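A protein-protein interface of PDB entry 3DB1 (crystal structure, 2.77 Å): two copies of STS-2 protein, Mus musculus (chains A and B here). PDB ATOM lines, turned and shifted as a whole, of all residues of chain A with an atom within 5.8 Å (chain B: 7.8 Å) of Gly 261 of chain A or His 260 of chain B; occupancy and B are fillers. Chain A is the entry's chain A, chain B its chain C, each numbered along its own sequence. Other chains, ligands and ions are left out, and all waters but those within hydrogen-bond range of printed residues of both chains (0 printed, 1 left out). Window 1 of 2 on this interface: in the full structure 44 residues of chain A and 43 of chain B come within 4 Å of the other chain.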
ATOM      1  N   GLU A  19      33.159  13.157 -13.694  1.00  0.00           N
ATOM      2  CA  GLU A  19      33.774  12.459 -14.810  1.00  0.00           C
ATOM      3  C   GLU A  19      35.097  13.099 -15.227  1.00  0.00           C
ATOM      4  O   GLU A  19      35.167  14.323 -15.475  1.00  0.00           O
ATOM      5  CB  GLU A  19      32.815  12.437 -16.005  1.00  0.00           C
ATOM      6  CG  GLU A  19      33.331  11.681 -17.189  1.00  0.00           C
ATOM      7  CD  GLU A  19      32.429  11.793 -18.388  1.00  0.00           C
ATOM      8  OE1 GLU A  19      32.397  12.882 -19.047  1.00  0.00           O
ATOM      9  OE2 GLU A  19      31.764  10.772 -18.704  1.00  0.00           O
ATOM     10  N   VAL A  24      36.686   8.891 -20.463  1.00  0.00           N
ATOM     11  CA  VAL A  24      35.969   8.820 -21.724  1.00  0.00           C
ATOM     12  C   VAL A  24      36.879   8.580 -22.900  1.00  0.00           C
ATOM     13  O   VAL A  24      36.515   7.827 -23.789  1.00  0.00           O
ATOM     14  CB  VAL A  24      35.150  10.082 -21.969  1.00  0.00           C
ATOM     15  CG1 VAL A  24      34.490  10.059 -23.312  1.00  0.00           C
ATOM     16  CG2 VAL A  24      34.093  10.217 -20.914  1.00  0.00           C
ATOM     17  N   ASN A  46      33.480  17.417 -25.203  1.00  0.00           N
ATOM     18  CA  ASN A  46      33.573  16.976 -23.852  1.00  0.00           C
ATOM     19  C   ASN A  46      34.920  17.257 -23.192  1.00  0.00           C
ATOM     20  O   ASN A  46      35.046  17.117 -21.965  1.00  0.00           O
ATOM     21  CB  ASN A  46      33.200  15.541 -23.713  1.00  0.00           C
ATOM     22  CG  ASN A  46      32.849  15.197 -22.298  1.00  0.00           C
ATOM     23  OD1 ASN A  46      32.310  16.041 -21.581  1.00  0.00           O
ATOM     24  ND2 ASN A  46      33.172  13.965 -21.860  1.00  0.00           N
ATOM     25  N   SER A  68      35.960  16.438 -17.338  1.00  0.00           N
ATOM     26  CA  SER A  68      35.443  16.630 -18.675  1.00  0.00           C
ATOM     27  C   SER A  68      34.377  17.718 -18.533  1.00  0.00           C
ATOM     28  O   SER A  68      34.077  18.145 -17.406  1.00  0.00           O
ATOM     29  CB  SER A  68      34.800  15.321 -19.165  1.00  0.00           C
ATOM     30  OG  SER A  68      33.723  14.907 -18.338  1.00  0.00           O
ATOM     31  N   CYS A  70      31.304  17.264 -19.064  1.00  0.00           N
ATOM     32  CA  CYS A  70      30.254  16.537 -18.357  1.00  0.00           C
ATOM     33  C   CYS A  70      30.568  16.520 -16.842  1.00  0.00           C
ATOM     34  O   CYS A  70      29.670  16.826 -16.004  1.00  0.00           O
ATOM     35  CB  CYS A  70      30.144  15.106 -18.884  1.00  0.00           C
ATOM     36  SG  CYS A  70      28.660  14.278 -18.345  1.00  0.00           S
ATOM     37  N   THR A 259      21.371  10.364 -12.292  1.00  0.00           N
ATOM     38  CA  THR A 259      21.405   9.308 -13.280  1.00  0.00           C
ATOM     39  C   THR A 259      21.210   9.918 -14.635  1.00  0.00           C
ATOM     40  O   THR A 259      20.220  10.638 -14.823  1.00  0.00           O
ATOM     41  CB  THR A 259      20.172   8.395 -13.059  1.00  0.00           C
ATOM     42  OG1 THR A 259      20.093   8.026 -11.686  1.00  0.00           O
ATOM     43  CG2 THR A 259      20.236   7.148 -13.933  1.00  0.00           C
ATOM     44  N   HIS A 260      22.078   9.593 -15.602  1.00  0.00           N
ATOM     45  CA  HIS A 260      21.866  10.050 -17.005  1.00  0.00           C
ATOM     46  C   HIS A 260      22.595   9.126 -17.966  1.00  0.00           C
ATOM     47  O   HIS A 260      23.480   8.419 -17.550  1.00  0.00           O
ATOM     48  CB  HIS A 260      22.319  11.540 -17.209  1.00  0.00           C
ATOM     49  CG  HIS A 260      23.809  11.743 -17.070  1.00  0.00           C
ATOM     50  ND1 HIS A 260      24.717  11.281 -18.004  1.00  0.00           N
ATOM     51  CD2 HIS A 260      24.547  12.325 -16.093  1.00  0.00           C
ATOM     52  CE1 HIS A 260      25.947  11.582 -17.597  1.00  0.00           C
ATOM     53  NE2 HIS A 260      25.868  12.204 -16.437  1.00  0.00           N
ATOM     54  N   GLY A 261      22.232   9.179 -19.252  1.00  0.00           N
ATOM     55  CA  GLY A 261      22.816   8.309 -20.306  1.00  0.00           C
ATOM     56  C   GLY A 261      24.106   8.861 -20.908  1.00  0.00           C
ATOM     57  O   GLY A 261      24.527  10.014 -20.619  1.00  0.00           O
ATOM     58  N   ALA A 262      24.749   8.032 -21.721  1.00  0.00           N
ATOM     59  CA  ALA A 262      25.956   8.430 -22.385  1.00  0.00           C
ATOM     60  C   ALA A 262      25.574   9.188 -23.644  1.00  0.00           C
ATOM     61  O   ALA A 262      24.402   9.400 -23.944  1.00  0.00           O
ATOM     62  CB  ALA A 262      26.778   7.218 -22.741  1.00  0.00           C
ATOM     63  N   ASN A 263      26.595   9.595 -24.380  1.00  0.00           N
ATOM     64  CA  ASN A 263      26.385  10.221 -25.634  1.00  0.00           C
ATOM     65  C   ASN A 263      27.526   9.771 -26.516  1.00  0.00           C
ATOM     66  O   ASN A 263      28.683  10.143 -26.265  1.00  0.00           O
ATOM     67  CB  ASN A 263      26.353  11.727 -25.455  1.00  0.00           C
ATOM     68  CG  ASN A 263      25.613  12.416 -26.580  1.00  0.00           C
ATOM     69  OD1 ASN A 263      26.213  13.163 -27.338  1.00  0.00           O
ATOM     70  ND2 ASN A 263      24.294  12.152 -26.715  1.00  0.00           N
ATOM     71  N   SER A 264      27.210   8.941 -27.516  1.00  0.00           N
ATOM     72  CA  SER A 264      28.271   8.233 -28.244  1.00  0.00           C
ATOM     73  C   SER A 264      28.753   9.076 -29.398  1.00  0.00           C
ATOM     74  O   SER A 264      28.037   9.971 -29.858  1.00  0.00           O
ATOM     75  CB  SER A 264      27.824   6.840 -28.714  1.00  0.00           C
ATOM     76  OG  SER A 264      26.635   6.918 -29.484  1.00  0.00           O
ATOM     77  N   GLU B  19      19.089  15.235 -24.430  1.00  0.00           N
ATOM     78  CA  GLU B  19      18.520  14.096 -23.758  1.00  0.00           C
ATOM     79  C   GLU B  19      17.190  14.422 -23.127  1.00  0.00           C
ATOM     80  O   GLU B  19      17.090  15.409 -22.410  1.00  0.00           O
ATOM     81  CB  GLU B  19      19.478  13.617 -22.672  1.00  0.00           C
ATOM     82  CG  GLU B  19      19.011  12.351 -21.955  1.00  0.00           C
ATOM     83  CD  GLU B  19      19.896  12.003 -20.793  1.00  0.00           C
ATOM     84  OE1 GLU B  19      19.784  12.663 -19.752  1.00  0.00           O
ATOM     85  OE2 GLU B  19      20.713  11.077 -20.889  1.00  0.00           O
ATOM     86  N   GLN B  23      13.879   9.125 -21.896  1.00  0.00           N
ATOM     87  CA  GLN B  23      14.955   8.303 -22.458  1.00  0.00           C
ATOM     88  C   GLN B  23      15.722   7.670 -21.288  1.00  0.00           C
ATOM     89  O   GLN B  23      16.323   6.602 -21.431  1.00  0.00           O
ATOM     90  CB  GLN B  23      15.895   9.219 -23.230  1.00  0.00           C
ATOM     91  CG  GLN B  23      16.742   8.646 -24.384  1.00  0.00           C
ATOM     92  CD  GLN B  23      17.537   9.790 -25.151  1.00  0.00           C
ATOM     93  OE1 GLN B  23      16.983  10.865 -25.545  1.00  0.00           O
ATOM     94  NE2 GLN B  23      18.832   9.543 -25.347  1.00  0.00           N
ATOM     95  N   VAL B  24      15.709   8.325 -20.122  1.00  0.00           N
ATOM     96  CA  VAL B  24      16.452   7.827 -18.960  1.00  0.00           C
ATOM     97  C   VAL B  24      15.594   7.084 -17.938  1.00  0.00           C
ATOM     98  O   VAL B  24      16.004   6.042 -17.403  1.00  0.00           O
ATOM     99  CB  VAL B  24      17.186   8.938 -18.241  1.00  0.00           C
ATOM    100  CG1 VAL B  24      17.919   8.374 -17.018  1.00  0.00           C
ATOM    101  CG2 VAL B  24      18.146   9.629 -19.196  1.00  0.00           C
ATOM    102  N   ASN B  46      18.644  14.313 -12.262  1.00  0.00           N
ATOM    103  CA  ASN B  46      18.592  14.460 -13.694  1.00  0.00           C
ATOM    104  C   ASN B  46      17.255  14.970 -14.134  1.00  0.00           C
ATOM    105  O   ASN B  46      17.114  15.440 -15.248  1.00  0.00           O
ATOM    106  CB  ASN B  46      18.949  13.182 -14.438  1.00  0.00           C
ATOM    107  CG  ASN B  46      19.317  13.451 -15.920  1.00  0.00           C
ATOM    108  OD1 ASN B  46      19.847  14.520 -16.286  1.00  0.00           O
ATOM    109  ND2 ASN B  46      19.060  12.479 -16.755  1.00  0.00           N
ATOM    110  N   SER B  68      16.175  16.505 -19.851  1.00  0.00           N
ATOM    111  CA  SER B  68      16.731  16.147 -18.566  1.00  0.00           C
ATOM    112  C   SER B  68      17.725  17.213 -18.241  1.00  0.00           C
ATOM    113  O   SER B  68      17.988  18.061 -19.065  1.00  0.00           O
ATOM    114  CB  SER B  68      17.455  14.797 -18.668  1.00  0.00           C
ATOM    115  OG  SER B  68      18.511  14.817 -19.623  1.00  0.00           O
ATOM    116  N   CYS B  70      20.824  16.691 -17.997  1.00  0.00           N
ATOM    117  CA  CYS B  70      21.891  16.385 -18.939  1.00  0.00           C
ATOM    118  C   CYS B  70      21.592  17.012 -20.320  1.00  0.00           C
ATOM    119  O   CYS B  70      22.421  17.735 -20.922  1.00  0.00           O
ATOM    120  CB  CYS B  70      22.036  14.872 -19.060  1.00  0.00           C
ATOM    121  SG  CYS B  70      23.599  14.377 -19.635  1.00  0.00           S
ATOM    122  N   GLY B  71      20.382  16.752 -20.803  1.00  0.00           N
ATOM    123  CA  GLY B  71      19.841  17.432 -21.979  1.00  0.00           C
ATOM    124  C   GLY B  71      20.175  18.906 -21.968  1.00  0.00           C
ATOM    125  O   GLY B  71      20.746  19.398 -22.935  1.00  0.00           O
ATOM    126  N   PHE B  73      22.471  20.494 -20.209  1.00  0.00           N
ATOM    127  CA  PHE B  73      23.921  20.613 -20.302  1.00  0.00           C
ATOM    128  C   PHE B  73      24.396  20.451 -21.748  1.00  0.00           C
ATOM    129  O   PHE B  73      25.180  21.276 -22.266  1.00  0.00           O
ATOM    130  CB  PHE B  73      24.592  19.621 -19.374  1.00  0.00           C
ATOM    131  CG  PHE B  73      25.864  19.086 -19.880  1.00  0.00           C
ATOM    132  CD1 PHE B  73      26.993  19.897 -19.930  1.00  0.00           C
ATOM    133  CD2 PHE B  73      25.958  17.766 -20.292  1.00  0.00           C
ATOM    134  CE1 PHE B  73      28.248  19.423 -20.425  1.00  0.00           C
ATOM    135  CE2 PHE B  73      27.213  17.272 -20.797  1.00  0.00           C
ATOM    136  CZ  PHE B  73      28.360  18.119 -20.831  1.00  0.00           C
ATOM    137  N   GLN B  74      23.870  19.429 -22.403  1.00  0.00           N
ATOM    138  CA  GLN B  74      24.196  19.207 -23.788  1.00  0.00           C
ATOM    139  C   GLN B  74      23.840  20.447 -24.656  1.00  0.00           C
ATOM    140  O   GLN B  74      24.640  20.885 -25.510  1.00  0.00           O
ATOM    141  CB  GLN B  74      23.492  17.944 -24.306  1.00  0.00           C
ATOM    142  CG  GLN B  74      23.990  16.702 -23.593  1.00  0.00           C
ATOM    143  CD  GLN B  74      23.144  15.444 -23.793  1.00  0.00           C
ATOM    144  OE1 GLN B  74      21.985  15.506 -24.222  1.00  0.00           O
ATOM    145  NE2 GLN B  74      23.727  14.292 -23.459  1.00  0.00           N
ATOM    146  N   LEU B  77      26.266  23.338 -23.926  1.00  0.00           N
ATOM    147  CA  LEU B  77      27.626  23.079 -24.376  1.00  0.00           C
ATOM    148  C   LEU B  77      27.742  23.309 -25.882  1.00  0.00           C
ATOM    149  O   LEU B  77      28.725  23.913 -26.359  1.00  0.00           O
ATOM    150  CB  LEU B  77      28.042  21.666 -24.014  1.00  0.00           C
ATOM    151  CG  LEU B  77      29.503  21.278 -24.132  1.00  0.00           C
ATOM    152  CD1 LEU B  77      30.411  21.979 -23.086  1.00  0.00           C
ATOM    153  CD2 LEU B  77      29.659  19.807 -24.072  1.00  0.00           C
ATOM    154  N   SER B 233      22.210  12.955 -28.989  1.00  0.00           N
ATOM    155  CA  SER B 233      21.756  14.261 -28.574  1.00  0.00           C
ATOM    156  C   SER B 233      22.713  15.354 -29.063  1.00  0.00           C
ATOM    157  O   SER B 233      23.955  15.164 -29.019  1.00  0.00           O
ATOM    158  CB  SER B 233      21.631  14.314 -27.068  1.00  0.00           C
ATOM    159  OG  SER B 233      20.913  13.187 -26.627  1.00  0.00           O
ATOM    160  N   THR B 257      31.848  17.151 -32.197  1.00  0.00           N
ATOM    161  CA  THR B 257      30.887  16.226 -31.609  1.00  0.00           C
ATOM    162  C   THR B 257      30.946  16.239 -30.064  1.00  0.00           C
ATOM    163  O   THR B 257      31.932  16.704 -29.487  1.00  0.00           O
ATOM    164  CB  THR B 257      31.082  14.811 -32.169  1.00  0.00           C
ATOM    165  OG1 THR B 257      30.088  13.970 -31.577  1.00  0.00           O
ATOM    166  CG2 THR B 257      32.472  14.268 -31.852  1.00  0.00           C
ATOM    167  N   LEU B 258      29.910  15.740 -29.396  1.00  0.00           N
ATOM    168  CA  LEU B 258      29.930  15.669 -27.932  1.00  0.00           C
ATOM    169  C   LEU B 258      29.842  14.233 -27.402  1.00  0.00           C
ATOM    170  O   LEU B 258      28.787  13.604 -27.481  1.00  0.00           O
ATOM    171  CB  LEU B 258      28.815  16.537 -27.364  1.00  0.00           C
ATOM    172  CG  LEU B 258      28.491  16.339 -25.871  1.00  0.00           C
ATOM    173  CD1 LEU B 258      29.694  16.489 -24.867  1.00  0.00           C
ATOM    174  CD2 LEU B 258      27.363  17.257 -25.459  1.00  0.00           C
ATOM    175  N   THR B 259      30.946  13.711 -26.865  1.00  0.00           N
ATOM    176  CA  THR B 259      30.990  12.310 -26.416  1.00  0.00           C
ATOM    177  C   THR B 259      31.173  12.267 -24.892  1.00  0.00           C
ATOM    178  O   THR B 259      32.150  12.843 -24.410  1.00  0.00           O
ATOM    179  CB  THR B 259      32.185  11.590 -27.028  1.00  0.00           C
ATOM    180  OG1 THR B 259      32.197  11.811 -28.421  1.00  0.00           O
ATOM    181  CG2 THR B 259      32.123  10.094 -26.802  1.00  0.00           C
ATOM    182  N   HIS B 260      30.283  11.588 -24.147  1.00  0.00           N
ATOM    183  CA  HIS B 260      30.463  11.410 -22.704  1.00  0.00           C
ATOM    184  C   HIS B 260      29.719  10.165 -22.188  1.00  0.00           C
ATOM    185  O   HIS B 260      28.775   9.679 -22.851  1.00  0.00           O
ATOM    186  CB  HIS B 260      30.000  12.635 -21.923  1.00  0.00           C
ATOM    187  CG  HIS B 260      28.521  12.838 -21.971  1.00  0.00           C
ATOM    188  ND1 HIS B 260      27.636  11.948 -21.402  1.00  0.00           N
ATOM    189  CD2 HIS B 260      27.769  13.781 -22.583  1.00  0.00           C
ATOM    190  CE1 HIS B 260      26.402  12.353 -21.639  1.00  0.00           C
ATOM    191  NE2 HIS B 260      26.454  13.458 -22.360  1.00  0.00           N
ATOM    192  N   GLY B 261      30.116   9.683 -21.001  1.00  0.00           N
ATOM    193  CA  GLY B 261      29.626   8.429 -20.462  1.00  0.00           C
ATOM    194  C   GLY B 261      28.336   8.579 -19.726  1.00  0.00           C
ATOM    195  O   GLY B 261      27.859   9.704 -19.458  1.00  0.00           O
ATOM    196  N   ALA B 262      27.736   7.450 -19.384  1.00  0.00           N
ATOM    197  CA  ALA B 262      26.519   7.507 -18.580  1.00  0.00           C
ATOM    198  C   ALA B 262      26.872   7.744 -17.097  1.00  0.00           C
ATOM    199  O   ALA B 262      28.039   7.733 -16.707  1.00  0.00           O
ATOM    200  CB  ALA B 262      25.727   6.201 -18.740  1.00  0.00           C
ATOM    201  N   ASN B 263      25.860   7.923 -16.271  1.00  0.00           N
ATOM    202  CA  ASN B 263      26.066   7.887 -14.867  1.00  0.00           C
ATOM    203  C   ASN B 263      24.949   7.029 -14.264  1.00  0.00           C
ATOM    204  O   ASN B 263      23.779   7.418 -14.319  1.00  0.00           O
ATOM    205  CB  ASN B 263      26.091   9.330 -14.372  1.00  0.00           C
ATOM    206  CG  ASN B 263      26.840   9.512 -13.067  1.00  0.00           C
ATOM    207  OD1 ASN B 263      26.241   9.886 -12.102  1.00  0.00           O
ATOM    208  ND2 ASN B 263      28.138   9.294 -13.049  1.00  0.00           N
ATOM    209  N   SER B 264      25.302   5.851 -13.738  1.00  0.00           N
ATOM    210  CA  SER B 264      24.286   4.876 -13.322  1.00  0.00           C
ATOM    211  C   SER B 264      23.773   5.165 -11.923  1.00  0.00           C
ATOM    212  O   SER B 264      24.445   5.804 -11.145  1.00  0.00           O
ATOM    213  CB  SER B 264      24.799   3.445 -13.458  1.00  0.00           C
ATOM    214  OG  SER B 264      25.978   3.274 -12.713  1.00  0.00           O
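Of the 11 printed residues of chain A, 9 touch a printed residue of chain B.
Hydrophobic or aromatic side chains of chain A within 4 Å of the printed part of chain B: Val 24, His 260 and Ala 262.
Along chain A the printed residues that touch a printed residue of chain B span positions 19 to 263.
Among the printed residues, no Asp or Glu carboxylate lies within 4 Å of a Lys or Arg side-chain nitrogen of the other chain.
Of chain B, only Glu 19 (2.9 Å), His 260 (3.2 Å), Gly 261 (3.5 Å) and Ala 262 (3.6 Å) come within 4 Å of Gly 261 of chain A.
His 260 of chain B touches just these residues of chain A: Glu 19, Asn 46, Cys 70, Gly 261, Ala 262 and Asn 263.
Printed residues of chain A within 4 Å of Cys 70 of chain B: His 260 (3.7 Å).
Printed residues of chain B within 4 Å of Val 24 of chain A: Thr 259.
Of the printed residues of chain B, Thr 259 of chain A touches Val 24 (3.9 Å), Asn 46 (2.9 Å) and Asn 263 (3.2 Å).
Of the printed residues of chain A, Gln 74 of chain B touches Asn 263.
Printed residues of chain B within 4 Å of Cys 70 of chain A: Phe 73 (3.5 Å) and His 260 (3.9 Å).
Gln 23 of chain B touches none of the printed residues of chain A.
The nearest residue of chain B that does not touch Gly 261 of chain A is Val 24 of chain B (4.1 Å).
The nearest residue of chain A that does not touch His 260 of chain B is His 260 of chain A (4.1 Å).
ND2 of Asn 46 of chain A lies within hydrogen-bond range of OE1 of Glu 19 of chain A.
OE1 of Glu 19 of chain A lies within hydrogen-bond range of OG of Ser 68 of chain A, at 2.5 Å.
OE1 of Glu 19 of chain B lies within hydrogen-bond range of OG of Ser 68 of chain B, at 2.5 Å.
The backbone NH of Glu 19 of chain B is in hydrogen-bond range of the side-chain amide oxygen of Gln 74 of chain B.
The side-chain hydroxyl of Ser 68 of chain B lies close to the backbone NH of Cys 70 of chain B (3.4 Å).
NE2 of His 260 of chain B lies within hydrogen-bond range of NE2 of Gln 74 of chain B (3.1 Å).
Among the printed residues, pairs that only touch across the chains: Glu 19 of chain A with His 260 of chain B (3.8 Å), Val 24 of chain A with Thr 259 of chain B (3.8 Å), Asn 46 of chain A with Leu 258 of chain B (3.8 Å), Asn 46 of chain A with His 260 of chain B (3.4 Å), Cys 70 of chain A with Phe 73 of chain B (3.5 Å), Cys 70 of chain A with His 260 of chain B (3.9 Å), Thr 259 of chain A with Val 24 of chain B (3.9 Å), Thr 259 of chain A with Asn 263 of chain B (3.2 Å), His 260 of chain A with Glu 19 of chain B (3.8 Å), His 260 of chain A with Asn 46 of chain B (3.4 Å), His 260 of chain A with Gly 261 of chain B (3.3 Å), His 260 of chain A with Ala 262 of chain B (3.3 Å), Gly 261 of chain A with His 260 of chain B (3.2 Å), Gly 261 of chain A with Gly 261 of chain B (3.5 Å), Gly 261 of chain A with Ala 262 of chain B (3.6 Å), Ala 262 of chain A with His 260 of chain B (3.1 Å), Ala 262 of chain A with Gly 261 of chain B (3.6 Å), Ala 262 of chain A with Ala 262 of chain B (3.5 Å), Asn 263 of chain A with Gln 74 of chain B (3.9 Å) and Asn 263 of chain A with Thr 259 of chain B (3.2 Å).
N of Gly 261 of chain B is in hydrogen-bond range of OE2 of Glu 19 of chain A (3.0 Å).
The backbone carbonyl oxygen (O) of Thr 259 of chain B lies within hydrogen-bond range of the side-chain amide nitrogen (ND2) of Asn 46 of chain A (3.0 Å).
O of Thr 259 of chain A sits close to ND2 of Asn 46 of chain B (2.9 Å).
A ring nitrogen (ND1) of His 260 of chain A lies within hydrogen-bond range of the side-chain sulfur of Cys 70 of chain B.
O of His 260 of chain A lies within hydrogen-bond range of N of Asn 263 of chain B, 2.7 Å away.
N of Gly 261 of chain A is in hydrogen-bond range of OE2 of Glu 19 of chain B (2.9 Å).
ND2 of Asn 263 of chain A lies close to N of Ser 233 of chain B.
The backbone carbonyl oxygen (O) of Leu 258 of chain B lies close to the side-chain amide oxygen (OD1) of Asn 263 of chain A.
N of Asn 263 of chain A sits at hydrogen-bond distance from O of His 260 of chain B, 2.7 Å away.
Glu 19 of chain A touches His 260 of chain B, and with the chains exchanged His 260 of chain A touches Glu 19 of chain B.
Thr 259 of chain A touches Asn 263 of chain B, and with the chains exchanged Asn 263 of chain A touches Thr 259 of chain B.
His 260 of chain A touches Gly 261 of chain B, and with the chains exchanged Gly 261 of chain A touches His 260 of chain B.
Gly 261 of chain A touches Ala 262 of chain B, and with the chains exchanged Ala 262 of chain A touches Gly 261 of chain B.
Positions printed for both chains: 19, 24, 46, 68, 70, 259, 260, 261, 262, 263 and 264.
Of the 29 pairs that touch across the chains among the printed residues, 24 have their exchanged pair printed and touching as well.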
